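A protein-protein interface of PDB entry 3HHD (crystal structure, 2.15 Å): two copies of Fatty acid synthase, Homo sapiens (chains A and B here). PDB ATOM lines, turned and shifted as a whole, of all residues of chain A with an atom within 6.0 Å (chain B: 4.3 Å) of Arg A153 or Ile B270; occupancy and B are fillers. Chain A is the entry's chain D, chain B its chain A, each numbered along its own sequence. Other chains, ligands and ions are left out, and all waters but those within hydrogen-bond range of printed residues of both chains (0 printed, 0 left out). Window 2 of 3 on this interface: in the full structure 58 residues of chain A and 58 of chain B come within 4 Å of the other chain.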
ATOM      1  N   ARG A 103      16.233  -6.627  26.871  1.00  0.00           N
ATOM      2  CA  ARG A 103      15.550  -7.650  26.087  1.00  0.00           C
ATOM      3  C   ARG A 103      15.894  -9.037  26.600  1.00  0.00           C
ATOM      4  O   ARG A 103      17.053  -9.309  26.873  1.00  0.00           O
ATOM      5  CB  ARG A 103      15.890  -7.527  24.601  1.00  0.00           C
ATOM      6  CG  ARG A 103      15.318  -6.303  23.935  1.00  0.00           C
ATOM      7  CD  ARG A 103      15.700  -6.262  22.452  1.00  0.00           C
ATOM      8  NE  ARG A 103      14.777  -7.056  21.606  1.00  0.00           N
ATOM      9  CZ  ARG A 103      13.540  -6.691  21.258  1.00  0.00           C
ATOM     10  NH1 ARG A 103      13.027  -5.529  21.657  1.00  0.00           N
ATOM     11  NH2 ARG A 103      12.782  -7.509  20.538  1.00  0.00           N
ATOM     12  N   GLY A 104      14.888  -9.903  26.744  1.00  0.00           N
ATOM     13  CA  GLY A 104      15.117 -11.267  27.179  1.00  0.00           C
ATOM     14  C   GLY A 104      15.213 -11.378  28.676  1.00  0.00           C
ATOM     15  O   GLY A 104      15.331 -12.483  29.216  1.00  0.00           O
ATOM     16  N   THR A 105      15.159 -10.238  29.371  1.00  0.00           N
ATOM     17  CA  THR A 105      15.201 -10.262  30.838  1.00  0.00           C
ATOM     18  C   THR A 105      13.786 -10.462  31.416  1.00  0.00           C
ATOM     19  O   THR A 105      12.762 -10.282  30.730  1.00  0.00           O
ATOM     20  CB  THR A 105      15.813  -8.993  31.442  1.00  0.00           C
ATOM     21  OG1 THR A 105      14.906  -7.899  31.287  1.00  0.00           O
ATOM     22  CG2 THR A 105      17.213  -8.666  30.856  1.00  0.00           C
ATOM     23  N   HIS A 106      13.753 -10.792  32.698  1.00  0.00           N
ATOM     24  CA  HIS A 106      12.506 -11.010  33.440  1.00  0.00           C
ATOM     25  C   HIS A 106      11.954  -9.682  33.955  1.00  0.00           C
ATOM     26  O   HIS A 106      11.320  -9.606  35.001  1.00  0.00           O
ATOM     27  CB  HIS A 106      12.731 -11.998  34.603  1.00  0.00           C
ATOM     28  CG  HIS A 106      11.513 -12.791  34.970  1.00  0.00           C
ATOM     29  ND1 HIS A 106      11.034 -13.825  34.190  1.00  0.00           N
ATOM     30  CD2 HIS A 106      10.639 -12.671  36.010  1.00  0.00           C
ATOM     31  CE1 HIS A 106       9.927 -14.310  34.736  1.00  0.00           C
ATOM     32  NE2 HIS A 106       9.668 -13.627  35.841  1.00  0.00           N
ATOM     33  N   THR A 107      12.103  -8.641  33.151  1.00  0.00           N
ATOM     34  CA  THR A 107      11.514  -7.335  33.469  1.00  0.00           C
ATOM     35  C   THR A 107       9.994  -7.485  33.416  1.00  0.00           C
ATOM     36  O   THR A 107       9.483  -8.161  32.519  1.00  0.00           O
ATOM     37  CB  THR A 107      12.007  -6.270  32.456  1.00  0.00           C
ATOM     38  OG1 THR A 107      13.379  -5.994  32.732  1.00  0.00           O
ATOM     39  CG2 THR A 107      11.210  -4.964  32.566  1.00  0.00           C
ATOM     40  N   GLY A 108       9.279  -6.899  34.380  1.00  0.00           N
ATOM     41  CA  GLY A 108       7.826  -6.994  34.403  1.00  0.00           C
ATOM     42  C   GLY A 108       7.132  -5.756  33.894  1.00  0.00           C
ATOM     43  O   GLY A 108       7.754  -4.695  33.776  1.00  0.00           O
ATOM     44  N   SER A 147       5.186  -5.861  26.554  1.00  0.00           N
ATOM     45  CA  SER A 147       6.101  -6.973  26.841  1.00  0.00           C
ATOM     46  C   SER A 147       6.578  -7.558  25.544  1.00  0.00           C
ATOM     47  O   SER A 147       7.749  -7.945  25.396  1.00  0.00           O
ATOM     48  CB  SER A 147       5.404  -8.050  27.670  1.00  0.00           C
ATOM     49  OG  SER A 147       5.021  -7.522  28.918  1.00  0.00           O
ATOM     50  N   ASP A 151      10.376  -7.084  24.441  1.00  0.00           N
ATOM     51  CA  ASP A 151      10.879  -8.417  24.775  1.00  0.00           C
ATOM     52  C   ASP A 151      11.085  -8.657  26.287  1.00  0.00           C
ATOM     53  O   ASP A 151      12.124  -9.143  26.710  1.00  0.00           O
ATOM     54  CB  ASP A 151      12.128  -8.760  23.958  1.00  0.00           C
ATOM     55  CG  ASP A 151      12.462 -10.253  24.006  1.00  0.00           C
ATOM     56  OD1 ASP A 151      11.550 -11.101  24.280  1.00  0.00           O
ATOM     57  OD2 ASP A 151      13.649 -10.588  23.797  1.00  0.00           O
ATOM     58  N   PHE A 152      10.080  -8.276  27.093  1.00  0.00           N
ATOM     59  CA  PHE A 152      10.133  -8.418  28.548  1.00  0.00           C
ATOM     60  C   PHE A 152       9.451  -9.726  28.899  1.00  0.00           C
ATOM     61  O   PHE A 152       8.367 -10.010  28.370  1.00  0.00           O
ATOM     62  CB  PHE A 152       9.389  -7.256  29.241  1.00  0.00           C
ATOM     63  CG  PHE A 152      10.028  -5.914  29.067  1.00  0.00           C
ATOM     64  CD1 PHE A 152      11.391  -5.802  28.848  1.00  0.00           C
ATOM     65  CD2 PHE A 152       9.273  -4.749  29.202  1.00  0.00           C
ATOM     66  CE1 PHE A 152      12.022  -4.548  28.767  1.00  0.00           C
ATOM     67  CE2 PHE A 152       9.881  -3.507  29.145  1.00  0.00           C
ATOM     68  CZ  PHE A 152      11.268  -3.411  28.910  1.00  0.00           C
ATOM     69  N   ARG A 153      10.075 -10.527  29.772  1.00  0.00           N
ATOM     70  CA  ARG A 153       9.531 -11.840  30.099  1.00  0.00           C
ATOM     71  C   ARG A 153       9.021 -11.984  31.514  1.00  0.00           C
ATOM     72  O   ARG A 153       8.629 -13.074  31.903  1.00  0.00           O
ATOM     73  CB  ARG A 153      10.544 -12.943  29.800  1.00  0.00           C
ATOM     74  CG  ARG A 153      11.280 -12.689  28.483  1.00  0.00           C
ATOM     75  CD  ARG A 153      11.299 -13.879  27.590  1.00  0.00           C
ATOM     76  NE  ARG A 153      11.890 -13.570  26.293  1.00  0.00           N
ATOM     77  CZ  ARG A 153      12.946 -14.194  25.787  1.00  0.00           C
ATOM     78  NH1 ARG A 153      13.543 -15.161  26.470  1.00  0.00           N
ATOM     79  NH2 ARG A 153      13.416 -13.837  24.603  1.00  0.00           N
ATOM     80  N   GLY A 154       9.053 -10.914  32.292  1.00  0.00           N
ATOM     81  CA  GLY A 154       8.500 -10.988  33.635  1.00  0.00           C
ATOM     82  C   GLY A 154       6.973 -10.925  33.543  1.00  0.00           C
ATOM     83  O   GLY A 154       6.391 -11.019  32.452  1.00  0.00           O
ATOM     84  N   PRO A 155       6.294 -10.783  34.700  1.00  0.00           N
ATOM     85  CA  PRO A 155       4.818 -10.690  34.648  1.00  0.00           C
ATOM     86  C   PRO A 155       4.343  -9.537  33.715  1.00  0.00           C
ATOM     87  O   PRO A 155       5.005  -8.514  33.558  1.00  0.00           O
ATOM     88  CB  PRO A 155       4.415 -10.380  36.130  1.00  0.00           C
ATOM     89  CG  PRO A 155       5.621 -10.786  36.978  1.00  0.00           C
ATOM     90  CD  PRO A 155       6.863 -10.601  36.063  1.00  0.00           C
ATOM     91  N   ASN B 254       5.363 -16.049  33.591  1.00  0.00           N
ATOM     92  CA  ASN B 254       6.309 -15.387  32.736  1.00  0.00           C
ATOM     93  C   ASN B 254       5.522 -14.903  31.525  1.00  0.00           C
ATOM     94  O   ASN B 254       4.303 -15.087  31.479  1.00  0.00           O
ATOM     95  CB  ASN B 254       7.539 -16.238  32.412  1.00  0.00           C
ATOM     96  CG  ASN B 254       7.252 -17.362  31.442  1.00  0.00           C
ATOM     97  OD1 ASN B 254       6.164 -17.491  30.922  1.00  0.00           O
ATOM     98  ND2 ASN B 254       8.248 -18.201  31.219  1.00  0.00           N
ATOM     99  N   THR B 255       6.192 -14.223  30.611  1.00  0.00           N
ATOM    100  CA  THR B 255       5.556 -13.697  29.395  1.00  0.00           C
ATOM    101  C   THR B 255       6.437 -14.072  28.230  1.00  0.00           C
ATOM    102  O   THR B 255       7.647 -14.148  28.374  1.00  0.00           O
ATOM    103  CB  THR B 255       5.331 -12.166  29.510  1.00  0.00           C
ATOM    104  OG1 THR B 255       4.595 -11.919  30.715  1.00  0.00           O
ATOM    105  CG2 THR B 255       4.523 -11.639  28.340  1.00  0.00           C
ATOM    106  N   ASP B 256       5.819 -14.403  27.104  1.00  0.00           N
ATOM    107  CA  ASP B 256       6.547 -14.824  25.898  1.00  0.00           C
ATOM    108  C   ASP B 256       7.594 -13.820  25.412  1.00  0.00           C
ATOM    109  O   ASP B 256       8.636 -14.203  24.858  1.00  0.00           O
ATOM    110  CB  ASP B 256       5.557 -15.126  24.760  1.00  0.00           C
ATOM    111  CG  ASP B 256       4.752 -16.432  24.983  1.00  0.00           C
ATOM    112  OD1 ASP B 256       5.082 -17.219  25.893  1.00  0.00           O
ATOM    113  OD2 ASP B 256       3.822 -16.715  24.200  1.00  0.00           O
ATOM    114  N   SER B 267       4.340 -19.291  22.484  1.00  0.00           N
ATOM    115  CA  SER B 267       5.695 -19.839  22.512  1.00  0.00           C
ATOM    116  C   SER B 267       5.883 -21.020  23.475  1.00  0.00           C
ATOM    117  O   SER B 267       5.991 -20.845  24.694  1.00  0.00           O
ATOM    118  CB  SER B 267       6.727 -18.741  22.801  1.00  0.00           C
ATOM    119  OG  SER B 267       8.037 -19.293  22.947  1.00  0.00           O
ATOM    120  N   GLY B 268       5.976 -22.221  22.911  1.00  0.00           N
ATOM    121  CA  GLY B 268       6.212 -23.436  23.675  1.00  0.00           C
ATOM    122  C   GLY B 268       7.540 -23.372  24.423  1.00  0.00           C
ATOM    123  O   GLY B 268       7.649 -23.997  25.478  1.00  0.00           O
ATOM    124  N   ASP B 269       8.551 -22.667  23.875  1.00  0.00           N
ATOM    125  CA  ASP B 269       9.865 -22.586  24.517  1.00  0.00           C
ATOM    126  C   ASP B 269       9.789 -21.813  25.854  1.00  0.00           C
ATOM    127  O   ASP B 269      10.416 -22.187  26.844  1.00  0.00           O
ATOM    128  CB  ASP B 269      10.865 -21.880  23.612  1.00  0.00           C
ATOM    129  CG  ASP B 269      11.266 -22.740  22.401  1.00  0.00           C
ATOM    130  OD1 ASP B 269      11.336 -23.999  22.517  1.00  0.00           O
ATOM    131  OD2 ASP B 269      11.539 -22.147  21.330  1.00  0.00           O
ATOM    132  N   ILE B 270       9.052 -20.710  25.851  1.00  0.00           N
ATOM    133  CA  ILE B 270       8.872 -19.892  27.050  1.00  0.00           C
ATOM    134  C   ILE B 270       7.972 -20.633  28.067  1.00  0.00           C
ATOM    135  O   ILE B 270       8.258 -20.655  29.248  1.00  0.00           O
ATOM    136  CB  ILE B 270       8.330 -18.486  26.680  1.00  0.00           C
ATOM    137  CG1 ILE B 270       9.285 -17.824  25.691  1.00  0.00           C
ATOM    138  CG2 ILE B 270       8.209 -17.598  27.950  1.00  0.00           C
ATOM    139  CD1 ILE B 270      10.622 -17.441  26.309  1.00  0.00           C
ATOM    140  N   GLN B 271       6.911 -21.282  27.590  1.00  0.00           N
ATOM    141  CA  GLN B 271       6.051 -22.079  28.462  1.00  0.00           C
ATOM    142  C   GLN B 271       6.872 -23.172  29.131  1.00  0.00           C
ATOM    143  O   GLN B 271       6.711 -23.478  30.322  1.00  0.00           O
ATOM    144  CB  GLN B 271       4.892 -22.728  27.670  1.00  0.00           C
ATOM    145  CG  GLN B 271       3.953 -21.684  27.002  1.00  0.00           C
ATOM    146  CD  GLN B 271       3.051 -22.323  25.968  1.00  0.00           C
ATOM    147  OE1 GLN B 271       3.067 -23.530  25.811  1.00  0.00           O
ATOM    148  NE2 GLN B 271       2.298 -21.515  25.220  1.00  0.00           N
ATOM    149  N   GLU B 272       7.739 -23.802  28.352  1.00  0.00           N
ATOM    150  CA  GLU B 272       8.571 -24.877  28.878  1.00  0.00           C
ATOM    151  C   GLU B 272       9.477 -24.369  29.994  1.00  0.00           C
ATOM    152  O   GLU B 272       9.656 -25.031  30.993  1.00  0.00           O
ATOM    153  CB  GLU B 272       9.421 -25.467  27.727  1.00  0.00           C
ATOM    154  CG  GLU B 272      10.445 -26.511  28.185  1.00  0.00           C
ATOM    155  CD  GLU B 272      11.594 -26.694  27.192  1.00  0.00           C
ATOM    156  OE1 GLU B 272      11.454 -26.293  26.017  1.00  0.00           O
ATOM    157  OE2 GLU B 272      12.657 -27.229  27.586  1.00  0.00           O
ATOM    158  N   GLN B 273      10.086 -23.199  29.809  1.00  0.00           N
ATOM    159  CA  GLN B 273      10.966 -22.602  30.828  1.00  0.00           C
ATOM    160  C   GLN B 273      10.191 -22.303  32.113  1.00  0.00           C
ATOM    161  O   GLN B 273      10.700 -22.455  33.222  1.00  0.00           O
ATOM    162  CB  GLN B 273      11.560 -21.287  30.313  1.00  0.00           C
ATOM    163  CG  GLN B 273      12.569 -21.450  29.197  1.00  0.00           C
ATOM    164  CD  GLN B 273      12.952 -20.111  28.571  1.00  0.00           C
ATOM    165  OE1 GLN B 273      13.277 -20.038  27.383  1.00  0.00           O
ATOM    166  NE2 GLN B 273      12.853 -19.036  29.356  1.00  0.00           N
ATOM    167  N   LEU B 274       8.951 -21.865  31.966  1.00  0.00           N
ATOM    168  CA  LEU B 274       8.136 -21.574  33.150  1.00  0.00           C
ATOM    169  C   LEU B 274       7.924 -22.857  33.937  1.00  0.00           C
ATOM    170  O   LEU B 274       8.082 -22.901  35.156  1.00  0.00           O
ATOM    171  CB  LEU B 274       6.763 -20.990  32.731  1.00  0.00           C
ATOM    172  CG  LEU B 274       5.830 -20.678  33.914  1.00  0.00           C
ATOM    173  CD1 LEU B 274       6.535 -19.654  34.887  1.00  0.00           C
ATOM    174  CD2 LEU B 274       4.530 -20.143  33.386  1.00  0.00           C
ATOM    175  N   ASN B 401       1.800 -16.217  30.620  1.00  0.00           N
ATOM    176  CA  ASN B 401       1.695 -17.619  31.039  1.00  0.00           C
ATOM    177  C   ASN B 401       1.671 -17.822  32.546  1.00  0.00           C
ATOM    178  O   ASN B 401       2.455 -17.222  33.271  1.00  0.00           O
ATOM    179  CB  ASN B 401       2.862 -18.440  30.466  1.00  0.00           C
ATOM    180  CG  ASN B 401       3.082 -18.201  28.998  1.00  0.00           C
ATOM    181  OD1 ASN B 401       2.153 -18.299  28.205  1.00  0.00           O
ATOM    182  ND2 ASN B 401       4.336 -17.978  28.615  1.00  0.00           N
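The backbone carbonyl oxygen of Gly A154 is in hydrogen-bond range of the side-chain hydroxyl of Thr B255 (2.7 Å). The backbone carbonyl oxygen (O) of Arg A153 lies within hydrogen-bond range of the backbone NH (N) of Thr B255, 3.0 Å away.
OD2 of Asp B256 lies within hydrogen-bond range of N of Ser B267, at 3.1 Å. The backbone NH of Asn B401 sits at hydrogen-bond distance from the backbone carbonyl oxygen of Asn B254 (2.9 Å). A ring nitrogen (ND1) of His A106 sits close to the backbone carbonyl oxygen of Arg A153 (3.4 Å). The backbone carbonyl oxygen (O) of Thr A107 is in hydrogen-bond range of the backbone NH (N) of Gly A154. OG of Ser B267 lies close to N of Ile B270. OD1 of Asp B256 sits at hydrogen-bond distance from ND2 of Asn B401 (2.9 Å).
Among the printed residues, pairs that only touch across the chains: His A106 with Asn B254, Ser A147 with Thr B255, Phe A152 with Thr B255, Arg A153 with Asn B254, Arg A153 with Asp B256, Arg A153 with Ile B270 and Pro A155 with Thr B255.
Of the printed residues of chain B, Ser A147 touches Thr B255 (3.8 Å). Arg A153 touches just these residues of chain B: Asn B254, Thr B255, Asp B256 and Ile B270. Of the printed residues of chain A, Thr B255 touches Ser A147 (3.8 Å), Phe A152 (3.9 Å), Arg A153 (3.0 Å), Gly A154 (2.7 Å) and Pro A155 (3.8 Å). The nearest printed residue of chain B that does not touch His A106 is Thr B255 (5.6 Å).
Hydrophobic or aromatic side chains of chain A within 4 Å of the printed part of chain B: His A106. Among the printed residues, no Asp or Glu carboxylate lies within 4 Å of a Lys or Arg side-chain nitrogen of the other chain.
No position is printed for both chains.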
